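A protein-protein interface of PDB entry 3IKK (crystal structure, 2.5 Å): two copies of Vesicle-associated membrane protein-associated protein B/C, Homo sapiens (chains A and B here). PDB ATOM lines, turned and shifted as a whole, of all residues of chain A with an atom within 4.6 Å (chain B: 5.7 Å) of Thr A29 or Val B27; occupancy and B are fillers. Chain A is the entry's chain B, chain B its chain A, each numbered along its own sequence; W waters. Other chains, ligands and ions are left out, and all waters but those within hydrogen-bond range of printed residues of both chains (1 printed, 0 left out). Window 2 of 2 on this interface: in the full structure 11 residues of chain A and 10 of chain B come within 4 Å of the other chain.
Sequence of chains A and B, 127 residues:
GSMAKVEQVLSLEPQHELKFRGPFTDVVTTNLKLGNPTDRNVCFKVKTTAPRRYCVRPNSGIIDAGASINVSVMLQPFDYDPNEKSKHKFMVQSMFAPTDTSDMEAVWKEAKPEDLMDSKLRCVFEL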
ATOM      1  N   VAL A  27       8.616 -23.262   7.508  1.00  0.00           N
ATOM      2  CA  VAL A  27       8.875 -23.800   6.183  1.00  0.00           C
ATOM      3  C   VAL A  27       9.238 -25.272   6.293  1.00  0.00           C
ATOM      4  O   VAL A  27       9.959 -25.684   7.214  1.00  0.00           O
ATOM      5  CB  VAL A  27       9.989 -23.040   5.431  1.00  0.00           C
ATOM      6  CG1 VAL A  27      10.228 -23.664   4.081  1.00  0.00           C
ATOM      7  CG2 VAL A  27       9.628 -21.583   5.266  1.00  0.00           C
ATOM      8  N   VAL A  28       8.719 -26.057   5.353  1.00  0.00           N
ATOM      9  CA  VAL A  28       8.973 -27.483   5.290  1.00  0.00           C
ATOM     10  C   VAL A  28       9.576 -27.799   3.941  1.00  0.00           C
ATOM     11  O   VAL A  28       8.999 -27.460   2.905  1.00  0.00           O
ATOM     12  CB  VAL A  28       7.673 -28.296   5.379  1.00  0.00           C
ATOM     13  CG1 VAL A  28       7.939 -29.736   4.976  1.00  0.00           C
ATOM     14  CG2 VAL A  28       7.078 -28.225   6.778  1.00  0.00           C
ATOM     15  N   THR A  29      10.721 -28.469   3.946  1.00  0.00           N
ATOM     16  CA  THR A  29      11.402 -28.821   2.711  1.00  0.00           C
ATOM     17  C   THR A  29      11.341 -30.321   2.422  1.00  0.00           C
ATOM     18  O   THR A  29      11.546 -31.142   3.321  1.00  0.00           O
ATOM     19  CB  THR A  29      12.883 -28.441   2.789  1.00  0.00           C
ATOM     20  OG1 THR A  29      13.003 -27.072   3.187  1.00  0.00           O
ATOM     21  CG2 THR A  29      13.585 -28.689   1.436  1.00  0.00           C
ATOM     22  N   THR A  30      11.074 -30.682   1.171  1.00  0.00           N
ATOM     23  CA  THR A  30      11.390 -32.039   0.727  1.00  0.00           C
ATOM     24  C   THR A  30      12.215 -32.046  -0.582  1.00  0.00           C
ATOM     25  O   THR A  30      11.901 -31.290  -1.513  1.00  0.00           O
ATOM     26  CB  THR A  30      10.133 -32.940   0.607  1.00  0.00           C
ATOM     27  OG1 THR A  30      10.544 -34.313   0.478  1.00  0.00           O
ATOM     28  CG2 THR A  30       9.295 -32.551  -0.595  1.00  0.00           C
ATOM     29  N   ASN A  31      13.266 -32.873  -0.637  1.00  0.00           N
ATOM     30  CA  ASN A  31      14.058 -32.997  -1.857  1.00  0.00           C
ATOM     31  C   ASN A  31      13.392 -33.834  -2.940  1.00  0.00           C
ATOM     32  O   ASN A  31      12.715 -34.822  -2.678  1.00  0.00           O
ATOM     33  CB  ASN A  31      15.445 -33.597  -1.586  1.00  0.00           C
ATOM     34  CG  ASN A  31      16.319 -32.712  -0.704  1.00  0.00           C
ATOM     35  OD1 ASN A  31      16.034 -31.524  -0.477  1.00  0.00           O
ATOM     36  ND2 ASN A  31      17.411 -33.295  -0.210  1.00  0.00           N
ATOM     37  N   SER A  72      15.640 -28.924  -3.874  1.00  0.00           N
ATOM     38  CA  SER A  72      14.924 -28.506  -2.661  1.00  0.00           C
ATOM     39  C   SER A  72      13.551 -27.922  -2.994  1.00  0.00           C
ATOM     40  O   SER A  72      13.459 -26.938  -3.724  1.00  0.00           O
ATOM     41  CB  SER A  72      15.737 -27.463  -1.891  1.00  0.00           C
ATOM     42  OG  SER A  72      17.056 -27.923  -1.638  1.00  0.00           O
ATOM     43  N   VAL A  73      12.495 -28.536  -2.461  1.00  0.00           N
ATOM     44  CA  VAL A  73      11.116 -28.073  -2.651  1.00  0.00           C
ATOM     45  C   VAL A  73      10.523 -27.633  -1.320  1.00  0.00           C
ATOM     46  O   VAL A  73      10.166 -28.460  -0.474  1.00  0.00           O
ATOM     47  CB  VAL A  73      10.210 -29.154  -3.301  1.00  0.00           C
ATOM     48  CG1 VAL A  73       8.735 -28.777  -3.188  1.00  0.00           C
ATOM     49  CG2 VAL A  73      10.588 -29.360  -4.767  1.00  0.00           C
ATOM     50  N   MET A  74      10.408 -26.320  -1.150  1.00  0.00           N
ATOM     51  CA  MET A  74      10.088 -25.726   0.147  1.00  0.00           C
ATOM     52  C   MET A  74       8.646 -25.229   0.292  1.00  0.00           C
ATOM     53  O   MET A  74       8.156 -24.449  -0.515  1.00  0.00           O
ATOM     54  CB  MET A  74      11.063 -24.599   0.416  1.00  0.00           C
ATOM     55  CG  MET A  74      12.481 -25.041   0.120  1.00  0.00           C
ATOM     56  SD  MET A  74      13.628 -23.699  -0.161  1.00  0.00           S
ATOM     57  CE  MET A  74      13.146 -23.226  -1.824  1.00  0.00           C
ATOM     58  N   THR B  25      23.283 -28.119   7.062  1.00  0.00           N
ATOM     59  CA  THR B  25      23.030 -29.416   6.447  1.00  0.00           C
ATOM     60  C   THR B  25      21.781 -29.325   5.591  1.00  0.00           C
ATOM     61  O   THR B  25      21.766 -29.735   4.431  1.00  0.00           O
ATOM     62  CB  THR B  25      22.692 -30.499   7.516  1.00  0.00           C
ATOM     63  OG1 THR B  25      23.521 -30.352   8.678  1.00  0.00           O
ATOM     64  CG2 THR B  25      22.850 -31.904   6.931  1.00  0.00           C
ATOM     65  N   ASP B  26      20.721 -28.810   6.206  1.00  0.00           N
ATOM     66  CA  ASP B  26      19.427 -28.676   5.571  1.00  0.00           C
ATOM     67  C   ASP B  26      19.154 -27.235   5.178  1.00  0.00           C
ATOM     68  O   ASP B  26      20.006 -26.349   5.341  1.00  0.00           O
ATOM     69  CB  ASP B  26      18.333 -29.126   6.539  1.00  0.00           C
ATOM     70  CG  ASP B  26      17.254 -29.948   5.856  1.00  0.00           C
ATOM     71  OD1 ASP B  26      16.381 -29.376   5.148  1.00  0.00           O
ATOM     72  OD2 ASP B  26      17.286 -31.186   6.046  1.00  0.00           O
ATOM     73  N   VAL B  27      17.942 -27.005   4.684  1.00  0.00           N
ATOM     74  CA  VAL B  27      17.508 -25.660   4.400  1.00  0.00           C
ATOM     75  C   VAL B  27      17.216 -24.957   5.731  1.00  0.00           C
ATOM     76  O   VAL B  27      16.539 -25.494   6.616  1.00  0.00           O
ATOM     77  CB  VAL B  27      16.299 -25.629   3.450  1.00  0.00           C
ATOM     78  CG1 VAL B  27      16.075 -24.230   2.938  1.00  0.00           C
ATOM     79  CG2 VAL B  27      16.521 -26.544   2.284  1.00  0.00           C
ATOM     80  N   VAL B  28      17.772 -23.759   5.862  1.00  0.00           N
ATOM     81  CA  VAL B  28      17.643 -22.946   7.047  1.00  0.00           C
ATOM     82  C   VAL B  28      16.776 -21.759   6.617  1.00  0.00           C
ATOM     83  O   VAL B  28      16.896 -21.284   5.487  1.00  0.00           O
ATOM     84  CB  VAL B  28      19.039 -22.471   7.550  1.00  0.00           C
ATOM     85  CG1 VAL B  28      18.942 -21.865   8.918  1.00  0.00           C
ATOM     86  CG2 VAL B  28      20.036 -23.621   7.569  1.00  0.00           C
ATOM     87  N   THR B  29      15.904 -21.300   7.514  1.00  0.00           N
ATOM     88  CA  THR B  29      14.878 -20.311   7.208  1.00  0.00           C
ATOM     89  C   THR B  29      14.876 -19.265   8.321  1.00  0.00           C
ATOM     90  O   THR B  29      15.217 -19.568   9.464  1.00  0.00           O
ATOM     91  CB  THR B  29      13.481 -20.972   7.208  1.00  0.00           C
ATOM     92  OG1 THR B  29      13.540 -22.266   6.584  1.00  0.00           O
ATOM     93  CG2 THR B  29      12.439 -20.094   6.504  1.00  0.00           C
ATOM     94  N   MET B  74      15.064 -18.090   3.066  1.00  0.00           N
ATOM     95  CA  MET B  74      15.388 -19.506   3.111  1.00  0.00           C
ATOM     96  C   MET B  74      16.724 -19.787   2.435  1.00  0.00           C
ATOM     97  O   MET B  74      16.917 -19.438   1.258  1.00  0.00           O
ATOM     98  CB  MET B  74      14.281 -20.306   2.418  1.00  0.00           C
ATOM     99  CG  MET B  74      12.882 -20.070   3.002  1.00  0.00           C
ATOM    100  SD  MET B  74      11.508 -20.821   2.066  1.00  0.00           S
ATOM    101  CE  MET B  74      11.215 -19.634   0.765  1.00  0.00           C
ATOM    102  N   LEU B  75      17.633 -20.431   3.175  1.00  0.00           N
ATOM    103  CA  LEU B  75      18.991 -20.699   2.698  1.00  0.00           C
ATOM    104  C   LEU B  75      19.121 -22.161   2.292  1.00  0.00           C
ATOM    105  O   LEU B  75      18.648 -23.056   2.979  1.00  0.00           O
ATOM    106  CB  LEU B  75      19.993 -20.358   3.800  1.00  0.00           C
ATOM    107  CG  LEU B  75      21.501 -20.366   3.549  1.00  0.00           C
ATOM    108  CD1 LEU B  75      21.879 -19.723   2.228  1.00  0.00           C
ATOM    109  CD2 LEU B  75      22.197 -19.672   4.706  1.00  0.00           C
ATOM    110  N   GLN B  76      19.752 -22.413   1.161  1.00  0.00           N
ATOM    111  CA  GLN B  76      19.911 -23.787   0.713  1.00  0.00           C
ATOM    112  C   GLN B  76      21.040 -24.421   1.484  1.00  0.00           C
ATOM    113  O   GLN B  76      21.906 -23.714   2.006  1.00  0.00           O
ATOM    114  CB  GLN B  76      20.172 -23.846  -0.785  1.00  0.00           C
ATOM    115  CG  GLN B  76      19.008 -23.312  -1.600  1.00  0.00           C
ATOM    116  CD  GLN B  76      17.724 -24.119  -1.410  1.00  0.00           C
ATOM    117  OE1 GLN B  76      17.754 -25.352  -1.416  1.00  0.00           O
ATOM    118  NE2 GLN B  76      16.591 -23.422  -1.242  1.00  0.00           N
ATOM    119  N   PRO B  77      21.029 -25.758   1.570  1.00  0.00           N
ATOM    120  CA  PRO B  77      22.048 -26.493   2.321  1.00  0.00           C
ATOM    121  C   PRO B  77      23.426 -26.227   1.740  1.00  0.00           C
ATOM    122  O   PRO B  77      23.559 -25.998   0.532  1.00  0.00           O
ATOM    123  CB  PRO B  77      21.654 -27.957   2.103  1.00  0.00           C
ATOM    124  CG  PRO B  77      20.217 -27.922   1.687  1.00  0.00           C
ATOM    125  CD  PRO B  77      20.069 -26.656   0.905  1.00  0.00           C
HETATM  126  O   HOH W   1      16.585 -30.169   2.004  1.00  0.00           O
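The side-chain amide oxygen of Gln B76 is in hydrogen-bond range of the side-chain hydroxyl of Ser A72. NE2 of Gln B76 lies within hydrogen-bond range of SD of Met A74 (3.2 Å).
Thr B29 touches Val A27. Val A27 touches Met B74 (CG1 to SD, 3.7 Å). Val B27 touches Thr A29. SD of Met A74 touches CG1 of Val B27 (3.98 Å).
Printed residues of chain B within 4 Å of Val A27: Thr B29 and Met B74. Thr A29 touches just one residue of chain B: Val B27 (3.6 Å). Of the printed residues of chain B, Ser A72 touches Gln B76. Printed residues of chain B within 4 Å of Met A74: Val B27 and Gln B76. Printed residues of chain A within 4 Å of Val B27: Thr A29 (3.6 Å) and Met A74 (3.98 Å). Val B28 touches none of the printed residues of chain A. Of the printed residues of chain A, Met B74 touches Val A27. Printed residues of chain A within 4 Å of Gln B76: Ser A72 (2.7 Å) and Met A74 (3.2 Å). The nearest residue of chain B that does not touch Thr A29 is Asp B26 (4.3 Å). The nearest printed residue of chain A that does not touch Val B27 is Ser A72 (4.2 Å).
Hydrophobic or aromatic side chains of chain B within 4 Å of the printed part of chain A: Val B27 and Met B74. Hydrophobic or aromatic side chains of chain A within 4 Å of the printed part of chain B: Val A27 and Met A74. Among the printed residues, 6 pairs touch across the chains.
Val A27 touches Thr B29, and with the chains exchanged Thr A29 touches Val B27. Val A27 touches Met B74, and with the chains exchanged Met A74 touches Val B27. Of the 6 pairs that touch across the chains among the printed residues, 4 have their exchanged pair printed and touching as well.
Water W1 bridges OD1 of Asn A31 (2.9 Å) and OD1 of Asp B26 (3.2 Å).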
